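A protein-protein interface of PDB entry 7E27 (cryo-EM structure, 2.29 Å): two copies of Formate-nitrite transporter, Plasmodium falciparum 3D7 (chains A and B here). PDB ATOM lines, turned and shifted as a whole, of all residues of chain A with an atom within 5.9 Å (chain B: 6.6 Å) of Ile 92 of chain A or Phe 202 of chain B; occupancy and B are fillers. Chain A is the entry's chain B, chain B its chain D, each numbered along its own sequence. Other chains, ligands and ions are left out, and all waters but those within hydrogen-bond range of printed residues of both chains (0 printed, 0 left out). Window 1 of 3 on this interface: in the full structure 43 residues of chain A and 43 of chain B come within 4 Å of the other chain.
The side-chain sulfur (SG) of Cys 57 of chain A lies close to the backbone NH (N) of Ala 93 of chain A (3.7 Å). The side-chain sulfur of Cys 96 of chain A is in hydrogen-bond range of the backbone carbonyl oxygen of Ile 92 of chain A, 3.2 Å away. SG of Cys 99 of chain A lies close to O of Met 95 of chain A, 3.4 Å away. The side-chain hydroxyl of Ser 24 of chain B sits at hydrogen-bond distance from the side-chain hydroxyl of Thr 205 of chain B (2.8 Å). The backbone carbonyl oxygen of Tyr 201 of chain B lies within hydrogen-bond range of the side-chain hydroxyl of Thr 205 of chain B. The backbone carbonyl oxygen (O) of Gly 211 of chain B sits at hydrogen-bond distance from the side-chain hydroxyl (OG) of Ser 215 of chain B, at 2.6 Å.
Among the printed residues, pairs that only touch across the chains: Cys 57 of chain A with Phe 195 of chain B, Ile 92 of chain A with Phe 195 of chain B, Ile 92 of chain A with Phe 202 of chain B, Ile 92 of chain A with Ser 215 of chain B, Ile 92 of chain A with Phe 218 of chain B, Ile 92 of chain A with Ala 219 of chain B, Met 95 of chain A with Phe 202 of chain B, Met 95 of chain A with Leu 206 of chain B, Cys 96 of chain A with Leu 198 of chain B, Cys 96 of chain A with Phe 202 of chain B, Cys 99 of chain A with Ser 24 of chain B, Cys 99 of chain A with Tyr 201 of chain B and Cys 99 of chain A with Phe 202 of chain B.
Of chain B, only Phe 195 (3.97 Å), Phe 202 (3.97 Å), Ser 215 (3.9 Å), Phe 218 (3.7 Å) and Ala 219 (3.9 Å) come within 4 Å of Ile 92 of chain A. Of the printed residues of chain A, Phe 202 of chain B touches Ile 92, Met 95, Cys 96 and Cys 99. Printed residues of chain B within 4 Å of Met 95 of chain A: Phe 202 and Leu 206. Printed residues of chain A within 4 Å of Ala 219 of chain B: Ile 92. Of the printed residues of chain A, Ser 215 of chain B touches Ile 92. Phe 217 of chain B touches none of the printed residues of chain A. The nearest residue of chain B that does not touch Ile 92 of chain A is Ala 222 of chain B (4.4 Å). The nearest printed residue of chain A that does not touch Phe 202 of chain B is Ile 97 of chain A (5.9 Å). The nearest printed residue of chain B that does not touch Met 95 of chain A is Ser 215 of chain B (4.5 Å).
Hydrophobic or aromatic side chains of chain B that line the printed part of chain A: Phe 195, Leu 198, Tyr 201, Phe 202, Leu 206 and Phe 218. Printed residues of chain A that touch a printed residue of chain B: Cys 57, Ile 92, Met 95, Cys 96 and Cys 99. Among the printed residues, 13 pairs touch across the chains. Among the printed residues, no Asp or Glu carboxylate lies within 4 Å of a Lys or Arg side-chain nitrogen of the other chain.
No position is printed for both chains. Of the 13 pairs that touch across the chains among the printed residues, none has its exchanged pair printed and touching as well.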
ATOM      1  N   CYS A  57      17.480 -33.654 -10.343  1.00  0.00           N
ATOM      2  CA  CYS A  57      18.612 -32.844 -10.766  1.00  0.00           C
ATOM      3  C   CYS A  57      19.649 -33.684 -11.503  1.00  0.00           C
ATOM      4  O   CYS A  57      20.355 -33.174 -12.378  1.00  0.00           O
ATOM      5  CB  CYS A  57      19.202 -32.130  -9.559  1.00  0.00           C
ATOM      6  SG  CYS A  57      17.961 -31.104  -8.756  1.00  0.00           S
ATOM      7  N   THR A  89      25.281 -27.908 -13.684  1.00  0.00           N
ATOM      8  CA  THR A  89      23.836 -27.948 -13.490  1.00  0.00           C
ATOM      9  C   THR A  89      23.379 -28.891 -12.380  1.00  0.00           C
ATOM     10  O   THR A  89      22.202 -28.857 -12.008  1.00  0.00           O
ATOM     11  CB  THR A  89      23.160 -28.283 -14.818  1.00  0.00           C
ATOM     12  OG1 THR A  89      21.779 -27.906 -14.784  1.00  0.00           O
ATOM     13  CG2 THR A  89      23.302 -29.667 -15.138  1.00  0.00           C
ATOM     14  N   PHE A  90      24.259 -29.714 -11.827  1.00  0.00           N
ATOM     15  CA  PHE A  90      23.842 -30.513 -10.671  1.00  0.00           C
ATOM     16  C   PHE A  90      23.582 -29.830  -9.312  1.00  0.00           C
ATOM     17  O   PHE A  90      22.649 -30.272  -8.634  1.00  0.00           O
ATOM     18  CB  PHE A  90      24.845 -31.644 -10.443  1.00  0.00           C
ATOM     19  CG  PHE A  90      24.310 -32.741  -9.571  1.00  0.00           C
ATOM     20  CD1 PHE A  90      23.154 -33.414  -9.921  1.00  0.00           C
ATOM     21  CD2 PHE A  90      24.943 -33.079  -8.387  1.00  0.00           C
ATOM     22  CE1 PHE A  90      22.645 -34.413  -9.116  1.00  0.00           C
ATOM     23  CE2 PHE A  90      24.438 -34.077  -7.577  1.00  0.00           C
ATOM     24  CZ  PHE A  90      23.287 -34.746  -7.945  1.00  0.00           C
ATOM     25  N   PRO A  91      24.326 -28.801  -8.846  1.00  0.00           N
ATOM     26  CA  PRO A  91      24.219 -28.423  -7.417  1.00  0.00           C
ATOM     27  C   PRO A  91      22.919 -27.769  -6.964  1.00  0.00           C
ATOM     28  O   PRO A  91      22.844 -27.360  -5.800  1.00  0.00           O
ATOM     29  CB  PRO A  91      25.388 -27.449  -7.232  1.00  0.00           C
ATOM     30  CG  PRO A  91      26.316 -27.778  -8.282  1.00  0.00           C
ATOM     31  CD  PRO A  91      25.453 -28.055  -9.438  1.00  0.00           C
ATOM     32  N   ILE A  92      21.891 -27.668  -7.808  1.00  0.00           N
ATOM     33  CA  ILE A  92      20.624 -27.104  -7.360  1.00  0.00           C
ATOM     34  C   ILE A  92      19.842 -28.099  -6.494  1.00  0.00           C
ATOM     35  O   ILE A  92      18.886 -27.712  -5.807  1.00  0.00           O
ATOM     36  CB  ILE A  92      19.840 -26.604  -8.604  1.00  0.00           C
ATOM     37  CG1 ILE A  92      18.731 -25.612  -8.227  1.00  0.00           C
ATOM     38  CG2 ILE A  92      19.311 -27.761  -9.423  1.00  0.00           C
ATOM     39  CD1 ILE A  92      19.177 -24.501  -7.304  1.00  0.00           C
ATOM     40  N   ALA A  93      20.275 -29.367  -6.465  1.00  0.00           N
ATOM     41  CA  ALA A  93      19.646 -30.386  -5.626  1.00  0.00           C
ATOM     42  C   ALA A  93      19.788 -30.077  -4.143  1.00  0.00           C
ATOM     43  O   ALA A  93      18.897 -30.404  -3.352  1.00  0.00           O
ATOM     44  CB  ALA A  93      20.245 -31.756  -5.937  1.00  0.00           C
ATOM     45  N   PHE A  94      20.903 -29.448  -3.752  1.00  0.00           N
ATOM     46  CA  PHE A  94      21.096 -29.034  -2.366  1.00  0.00           C
ATOM     47  C   PHE A  94      20.040 -28.023  -1.938  1.00  0.00           C
ATOM     48  O   PHE A  94      19.484 -28.128  -0.840  1.00  0.00           O
ATOM     49  CB  PHE A  94      22.500 -28.451  -2.193  1.00  0.00           C
ATOM     50  CG  PHE A  94      23.035 -28.533  -0.788  1.00  0.00           C
ATOM     51  CD1 PHE A  94      22.611 -27.649   0.193  1.00  0.00           C
ATOM     52  CD2 PHE A  94      23.985 -29.481  -0.457  1.00  0.00           C
ATOM     53  CE1 PHE A  94      23.103 -27.726   1.472  1.00  0.00           C
ATOM     54  CE2 PHE A  94      24.484 -29.559   0.825  1.00  0.00           C
ATOM     55  CZ  PHE A  94      24.041 -28.681   1.789  1.00  0.00           C
ATOM     56  N   MET A  95      19.737 -27.053  -2.803  1.00  0.00           N
ATOM     57  CA  MET A  95      18.705 -26.068  -2.502  1.00  0.00           C
ATOM     58  C   MET A  95      17.321 -26.700  -2.490  1.00  0.00           C
ATOM     59  O   MET A  95      16.479 -26.338  -1.657  1.00  0.00           O
ATOM     60  CB  MET A  95      18.774 -24.925  -3.515  1.00  0.00           C
ATOM     61  CG  MET A  95      18.273 -23.582  -3.013  1.00  0.00           C
ATOM     62  SD  MET A  95      19.099 -22.984  -1.533  1.00  0.00           S
ATOM     63  CE  MET A  95      20.795 -23.094  -2.060  1.00  0.00           C
ATOM     64  N   CYS A  96      17.084 -27.655  -3.401  1.00  0.00           N
ATOM     65  CA  CYS A  96      15.824 -28.397  -3.411  1.00  0.00           C
ATOM     66  C   CYS A  96      15.616 -29.173  -2.114  1.00  0.00           C
ATOM     67  O   CYS A  96      14.489 -29.274  -1.618  1.00  0.00           O
ATOM     68  CB  CYS A  96      15.777 -29.356  -4.602  1.00  0.00           C
ATOM     69  SG  CYS A  96      15.866 -28.600  -6.233  1.00  0.00           S
ATOM     70  N   ILE A  97      16.691 -29.713  -1.542  1.00  0.00           N
ATOM     71  CA  ILE A  97      16.560 -30.501  -0.321  1.00  0.00           C
ATOM     72  C   ILE A  97      16.432 -29.592   0.901  1.00  0.00           C
ATOM     73  O   ILE A  97      15.599 -29.834   1.782  1.00  0.00           O
ATOM     74  CB  ILE A  97      17.735 -31.490  -0.197  1.00  0.00           C
ATOM     75  CG1 ILE A  97      17.601 -32.588  -1.250  1.00  0.00           C
ATOM     76  CG2 ILE A  97      17.789 -32.140   1.174  1.00  0.00           C
ATOM     77  CD1 ILE A  97      18.893 -33.265  -1.589  1.00  0.00           C
ATOM     78  N   CYS A  99      15.445 -26.391   1.130  1.00  0.00           N
ATOM     79  CA  CYS A  99      14.335 -25.451   1.211  1.00  0.00           C
ATOM     80  C   CYS A  99      13.020 -26.154   1.523  1.00  0.00           C
ATOM     81  O   CYS A  99      12.089 -25.522   2.029  1.00  0.00           O
ATOM     82  CB  CYS A  99      14.241 -24.635  -0.074  1.00  0.00           C
ATOM     83  SG  CYS A  99      15.553 -23.390  -0.220  1.00  0.00           S
ATOM     84  N   SER B  24       8.625 -21.961   5.753  1.00  0.00           N
ATOM     85  CA  SER B  24       8.483 -21.886   4.304  1.00  0.00           C
ATOM     86  C   SER B  24       7.155 -22.487   3.853  1.00  0.00           C
ATOM     87  O   SER B  24       6.494 -21.945   2.957  1.00  0.00           O
ATOM     88  CB  SER B  24       9.666 -22.585   3.642  1.00  0.00           C
ATOM     89  OG  SER B  24       9.646 -22.401   2.247  1.00  0.00           O
ATOM     90  N   PHE B 195      10.536 -28.566 -10.646  1.00  0.00           N
ATOM     91  CA  PHE B 195      11.490 -27.454 -10.586  1.00  0.00           C
ATOM     92  C   PHE B 195      10.801 -26.106 -10.409  1.00  0.00           C
ATOM     93  O   PHE B 195      11.311 -25.236  -9.690  1.00  0.00           O
ATOM     94  CB  PHE B 195      12.360 -27.380 -11.842  1.00  0.00           C
ATOM     95  CG  PHE B 195      13.587 -28.236 -11.811  1.00  0.00           C
ATOM     96  CD1 PHE B 195      14.611 -27.956 -10.924  1.00  0.00           C
ATOM     97  CD2 PHE B 195      13.781 -29.231 -12.750  1.00  0.00           C
ATOM     98  CE1 PHE B 195      15.759 -28.709 -10.914  1.00  0.00           C
ATOM     99  CE2 PHE B 195      14.945 -29.980 -12.752  1.00  0.00           C
ATOM    100  CZ  PHE B 195      15.931 -29.717 -11.829  1.00  0.00           C
ATOM    101  N   CYS B 197       7.805 -25.390  -8.972  1.00  0.00           N
ATOM    102  CA  CYS B 197       7.274 -25.235  -7.622  1.00  0.00           C
ATOM    103  C   CYS B 197       8.391 -25.168  -6.585  1.00  0.00           C
ATOM    104  O   CYS B 197       8.251 -24.497  -5.553  1.00  0.00           O
ATOM    105  CB  CYS B 197       6.304 -26.374  -7.329  1.00  0.00           C
ATOM    106  SG  CYS B 197       4.889 -26.395  -8.440  1.00  0.00           S
ATOM    107  N   LEU B 198       9.534 -25.799  -6.868  1.00  0.00           N
ATOM    108  CA  LEU B 198      10.685 -25.640  -5.989  1.00  0.00           C
ATOM    109  C   LEU B 198      11.263 -24.232  -6.068  1.00  0.00           C
ATOM    110  O   LEU B 198      11.728 -23.702  -5.062  1.00  0.00           O
ATOM    111  CB  LEU B 198      11.749 -26.682  -6.315  1.00  0.00           C
ATOM    112  CG  LEU B 198      11.485 -28.046  -5.678  1.00  0.00           C
ATOM    113  CD1 LEU B 198      12.245 -29.124  -6.407  1.00  0.00           C
ATOM    114  CD2 LEU B 198      11.846 -28.035  -4.216  1.00  0.00           C
ATOM    115  N   ALA B 199      11.231 -23.603  -7.246  1.00  0.00           N
ATOM    116  CA  ALA B 199      11.690 -22.217  -7.352  1.00  0.00           C
ATOM    117  C   ALA B 199      10.753 -21.257  -6.620  1.00  0.00           C
ATOM    118  O   ALA B 199      11.197 -20.245  -6.052  1.00  0.00           O
ATOM    119  CB  ALA B 199      11.829 -21.824  -8.821  1.00  0.00           C
ATOM    120  N   VAL B 200       9.454 -21.569  -6.615  1.00  0.00           N
ATOM    121  CA  VAL B 200       8.504 -20.819  -5.790  1.00  0.00           C
ATOM    122  C   VAL B 200       8.835 -20.977  -4.303  1.00  0.00           C
ATOM    123  O   VAL B 200       8.822 -20.001  -3.538  1.00  0.00           O
ATOM    124  CB  VAL B 200       7.061 -21.256  -6.116  1.00  0.00           C
ATOM    125  CG1 VAL B 200       6.063 -20.668  -5.132  1.00  0.00           C
ATOM    126  CG2 VAL B 200       6.693 -20.857  -7.534  1.00  0.00           C
ATOM    127  N   TYR B 201       9.175 -22.199  -3.880  1.00  0.00           N
ATOM    128  CA  TYR B 201       9.668 -22.422  -2.518  1.00  0.00           C
ATOM    129  C   TYR B 201      10.969 -21.670  -2.233  1.00  0.00           C
ATOM    130  O   TYR B 201      11.190 -21.213  -1.104  1.00  0.00           O
ATOM    131  CB  TYR B 201       9.850 -23.919  -2.274  1.00  0.00           C
ATOM    132  CG  TYR B 201       8.788 -24.524  -1.398  1.00  0.00           C
ATOM    133  CD1 TYR B 201       8.886 -24.451  -0.020  1.00  0.00           C
ATOM    134  CD2 TYR B 201       7.666 -25.122  -1.941  1.00  0.00           C
ATOM    135  CE1 TYR B 201       7.915 -24.989   0.800  1.00  0.00           C
ATOM    136  CE2 TYR B 201       6.686 -25.657  -1.127  1.00  0.00           C
ATOM    137  CZ  TYR B 201       6.818 -25.583   0.240  1.00  0.00           C
ATOM    138  OH  TYR B 201       5.847 -26.115   1.049  1.00  0.00           O
ATOM    139  N   PHE B 202      11.836 -21.535  -3.241  1.00  0.00           N
ATOM    140  CA  PHE B 202      13.099 -20.817  -3.068  1.00  0.00           C
ATOM    141  C   PHE B 202      12.856 -19.342  -2.791  1.00  0.00           C
ATOM    142  O   PHE B 202      13.482 -18.763  -1.899  1.00  0.00           O
ATOM    143  CB  PHE B 202      13.995 -20.954  -4.304  1.00  0.00           C
ATOM    144  CG  PHE B 202      14.488 -22.348  -4.581  1.00  0.00           C
ATOM    145  CD1 PHE B 202      14.468 -23.335  -3.609  1.00  0.00           C
ATOM    146  CD2 PHE B 202      14.981 -22.665  -5.837  1.00  0.00           C
ATOM    147  CE1 PHE B 202      14.902 -24.610  -3.893  1.00  0.00           C
ATOM    148  CE2 PHE B 202      15.432 -23.936  -6.118  1.00  0.00           C
ATOM    149  CZ  PHE B 202      15.395 -24.906  -5.145  1.00  0.00           C
ATOM    150  N   VAL B 203      11.951 -18.713  -3.547  1.00  0.00           N
ATOM    151  CA  VAL B 203      11.704 -17.293  -3.291  1.00  0.00           C
ATOM    152  C   VAL B 203      10.859 -17.103  -2.038  1.00  0.00           C
ATOM    153  O   VAL B 203      10.849 -16.014  -1.454  1.00  0.00           O
ATOM    154  CB  VAL B 203      11.066 -16.576  -4.498  1.00  0.00           C
ATOM    155  CG1 VAL B 203      12.066 -16.436  -5.610  1.00  0.00           C
ATOM    156  CG2 VAL B 203       9.814 -17.266  -4.965  1.00  0.00           C
ATOM    157  N   LEU B 204      10.145 -18.136  -1.594  1.00  0.00           N
ATOM    158  CA  LEU B 204       9.478 -18.023  -0.301  1.00  0.00           C
ATOM    159  C   LEU B 204      10.450 -18.202   0.861  1.00  0.00           C
ATOM    160  O   LEU B 204      10.167 -17.751   1.975  1.00  0.00           O
ATOM    161  CB  LEU B 204       8.341 -19.034  -0.202  1.00  0.00           C
ATOM    162  CG  LEU B 204       7.089 -18.649  -0.986  1.00  0.00           C
ATOM    163  CD1 LEU B 204       6.215 -19.855  -1.171  1.00  0.00           C
ATOM    164  CD2 LEU B 204       6.332 -17.538  -0.292  1.00  0.00           C
ATOM    165  N   THR B 205      11.593 -18.846   0.629  1.00  0.00           N
ATOM    166  CA  THR B 205      12.558 -19.099   1.695  1.00  0.00           C
ATOM    167  C   THR B 205      13.661 -18.043   1.767  1.00  0.00           C
ATOM    168  O   THR B 205      13.927 -17.496   2.839  1.00  0.00           O
ATOM    169  CB  THR B 205      13.178 -20.489   1.516  1.00  0.00           C
ATOM    170  OG1 THR B 205      12.140 -21.467   1.421  1.00  0.00           O
ATOM    171  CG2 THR B 205      14.080 -20.831   2.683  1.00  0.00           C
ATOM    172  N   LEU B 206      14.315 -17.751   0.647  1.00  0.00           N
ATOM    173  CA  LEU B 206      15.506 -16.908   0.630  1.00  0.00           C
ATOM    174  C   LEU B 206      15.110 -15.477   0.280  1.00  0.00           C
ATOM    175  O   LEU B 206      14.813 -15.174  -0.878  1.00  0.00           O
ATOM    176  CB  LEU B 206      16.526 -17.460  -0.361  1.00  0.00           C
ATOM    177  CG  LEU B 206      16.636 -18.986  -0.399  1.00  0.00           C
ATOM    178  CD1 LEU B 206      17.382 -19.440  -1.624  1.00  0.00           C
ATOM    179  CD2 LEU B 206      17.314 -19.510   0.846  1.00  0.00           C
ATOM    180  N   LYS B 207      15.107 -14.599   1.279  1.00  0.00           N
ATOM    181  CA  LYS B 207      14.594 -13.237   1.123  1.00  0.00           C
ATOM    182  C   LYS B 207      15.715 -12.224   0.881  1.00  0.00           C
ATOM    183  O   LYS B 207      15.822 -11.217   1.572  1.00  0.00           O
ATOM    184  CB  LYS B 207      13.776 -12.849   2.350  1.00  0.00           C
ATOM    185  CG  LYS B 207      12.709 -13.838   2.754  1.00  0.00           C
ATOM    186  CD  LYS B 207      11.761 -14.138   1.618  1.00  0.00           C
ATOM    187  CE  LYS B 207      10.591 -13.181   1.616  1.00  0.00           C
ATOM    188  NZ  LYS B 207       9.555 -13.592   0.635  1.00  0.00           N
ATOM    189  N   GLY B 211      19.446 -14.563  -3.446  1.00  0.00           N
ATOM    190  CA  GLY B 211      18.633 -15.765  -3.406  1.00  0.00           C
ATOM    191  C   GLY B 211      17.574 -15.776  -4.490  1.00  0.00           C
ATOM    192  O   GLY B 211      17.479 -16.747  -5.254  1.00  0.00           O
ATOM    193  N   TYR B 212      16.829 -14.659  -4.615  1.00  0.00           N
ATOM    194  CA  TYR B 212      15.806 -14.509  -5.653  1.00  0.00           C
ATOM    195  C   TYR B 212      16.366 -14.716  -7.049  1.00  0.00           C
ATOM    196  O   TYR B 212      15.779 -15.443  -7.850  1.00  0.00           O
ATOM    197  CB  TYR B 212      15.127 -13.136  -5.615  1.00  0.00           C
ATOM    198  CG  TYR B 212      13.966 -12.973  -4.666  1.00  0.00           C
ATOM    199  CD1 TYR B 212      13.730 -13.877  -3.647  1.00  0.00           C
ATOM    200  CD2 TYR B 212      12.999 -12.007  -4.917  1.00  0.00           C
ATOM    201  CE1 TYR B 212      12.640 -13.741  -2.819  1.00  0.00           C
ATOM    202  CE2 TYR B 212      11.897 -11.878  -4.116  1.00  0.00           C
ATOM    203  CZ  TYR B 212      11.725 -12.748  -3.063  1.00  0.00           C
ATOM    204  OH  TYR B 212      10.626 -12.620  -2.255  1.00  0.00           O
ATOM    205  N   PHE B 214      19.467 -16.063  -8.123  1.00  0.00           N
ATOM    206  CA  PHE B 214      20.280 -17.198  -8.521  1.00  0.00           C
ATOM    207  C   PHE B 214      19.687 -18.562  -8.194  1.00  0.00           C
ATOM    208  O   PHE B 214      19.980 -19.515  -8.930  1.00  0.00           O
ATOM    209  CB  PHE B 214      21.680 -17.057  -7.928  1.00  0.00           C
ATOM    210  CG  PHE B 214      22.528 -16.092  -8.687  1.00  0.00           C
ATOM    211  CD1 PHE B 214      22.918 -16.375  -9.987  1.00  0.00           C
ATOM    212  CD2 PHE B 214      22.886 -14.874  -8.133  1.00  0.00           C
ATOM    213  CE1 PHE B 214      23.682 -15.482 -10.703  1.00  0.00           C
ATOM    214  CE2 PHE B 214      23.652 -13.983  -8.845  1.00  0.00           C
ATOM    215  CZ  PHE B 214      24.048 -14.288 -10.130  1.00  0.00           C
ATOM    216  N   SER B 215      18.825 -18.692  -7.173  1.00  0.00           N
ATOM    217  CA  SER B 215      18.168 -19.981  -6.967  1.00  0.00           C
ATOM    218  C   SER B 215      17.207 -20.288  -8.105  1.00  0.00           C
ATOM    219  O   SER B 215      17.204 -21.402  -8.648  1.00  0.00           O
ATOM    220  CB  SER B 215      17.427 -20.004  -5.634  1.00  0.00           C
ATOM    221  OG  SER B 215      16.387 -19.066  -5.621  1.00  0.00           O
ATOM    222  N   VAL B 216      16.420 -19.290  -8.517  1.00  0.00           N
ATOM    223  CA  VAL B 216      15.486 -19.549  -9.600  1.00  0.00           C
ATOM    224  C   VAL B 216      16.212 -19.537 -10.932  1.00  0.00           C
ATOM    225  O   VAL B 216      15.738 -20.159 -11.886  1.00  0.00           O
ATOM    226  CB  VAL B 216      14.298 -18.567  -9.592  1.00  0.00           C
ATOM    227  CG1 VAL B 216      13.750 -18.412  -8.195  1.00  0.00           C
ATOM    228  CG2 VAL B 216      14.621 -17.244 -10.259  1.00  0.00           C
ATOM    229  N   PHE B 217      17.390 -18.894 -11.014  1.00  0.00           N
ATOM    230  CA  PHE B 217      18.219 -19.032 -12.206  1.00  0.00           C
ATOM    231  C   PHE B 217      18.630 -20.479 -12.412  1.00  0.00           C
ATOM    232  O   PHE B 217      18.430 -21.040 -13.494  1.00  0.00           O
ATOM    233  CB  PHE B 217      19.464 -18.143 -12.127  1.00  0.00           C
ATOM    234  CG  PHE B 217      20.478 -18.446 -13.200  1.00  0.00           C
ATOM    235  CD1 PHE B 217      20.256 -18.031 -14.504  1.00  0.00           C
ATOM    236  CD2 PHE B 217      21.633 -19.172 -12.918  1.00  0.00           C
ATOM    237  CE1 PHE B 217      21.160 -18.319 -15.501  1.00  0.00           C
ATOM    238  CE2 PHE B 217      22.534 -19.471 -13.916  1.00  0.00           C
ATOM    239  CZ  PHE B 217      22.298 -19.039 -15.208  1.00  0.00           C
ATOM    240  N   PHE B 218      19.184 -21.104 -11.369  1.00  0.00           N
ATOM    241  CA  PHE B 218      19.661 -22.472 -11.516  1.00  0.00           C
ATOM    242  C   PHE B 218      18.507 -23.456 -11.689  1.00  0.00           C
ATOM    243  O   PHE B 218      18.610 -24.385 -12.494  1.00  0.00           O
ATOM    244  CB  PHE B 218      20.553 -22.844 -10.335  1.00  0.00           C
ATOM    245  CG  PHE B 218      21.961 -22.340 -10.471  1.00  0.00           C
ATOM    246  CD1 PHE B 218      22.782 -22.803 -11.489  1.00  0.00           C
ATOM    247  CD2 PHE B 218      22.461 -21.393  -9.594  1.00  0.00           C
ATOM    248  CE1 PHE B 218      24.074 -22.338 -11.621  1.00  0.00           C
ATOM    249  CE2 PHE B 218      23.750 -20.923  -9.721  1.00  0.00           C
ATOM    250  CZ  PHE B 218      24.558 -21.398 -10.735  1.00  0.00           C
ATOM    251  N   ALA B 219      17.366 -23.211 -11.032  1.00  0.00           N
ATOM    252  CA  ALA B 219      16.214 -24.103 -11.185  1.00  0.00           C
ATOM    253  C   ALA B 219      15.594 -24.012 -12.582  1.00  0.00           C
ATOM    254  O   ALA B 219      15.307 -25.042 -13.216  1.00  0.00           O
ATOM    255  CB  ALA B 219      15.169 -23.788 -10.115  1.00  0.00           C
ATOM    256  N   VAL B 220      15.390 -22.791 -13.089  1.00  0.00           N
ATOM    257  CA  VAL B 220      14.712 -22.629 -14.368  1.00  0.00           C
ATOM    258  C   VAL B 220      15.638 -23.008 -15.517  1.00  0.00           C
ATOM    259  O   VAL B 220      15.206 -23.653 -16.484  1.00  0.00           O
ATOM    260  CB  VAL B 220      14.149 -21.199 -14.495  1.00  0.00           C
ATOM    261  CG1 VAL B 220      13.623 -20.925 -15.890  1.00  0.00           C
ATOM    262  CG2 VAL B 220      13.026 -21.001 -13.498  1.00  0.00           C
ATOM    263  N   ALA B 222      17.849 -25.301 -15.157  1.00  0.00           N
ATOM    264  CA  ALA B 222      17.927 -26.750 -15.042  1.00  0.00           C
ATOM    265  C   ALA B 222      16.766 -27.436 -15.748  1.00  0.00           C
ATOM    266  O   ALA B 222      16.969 -28.445 -16.427  1.00  0.00           O
ATOM    267  CB  ALA B 222      17.980 -27.157 -13.571  1.00  0.00           C
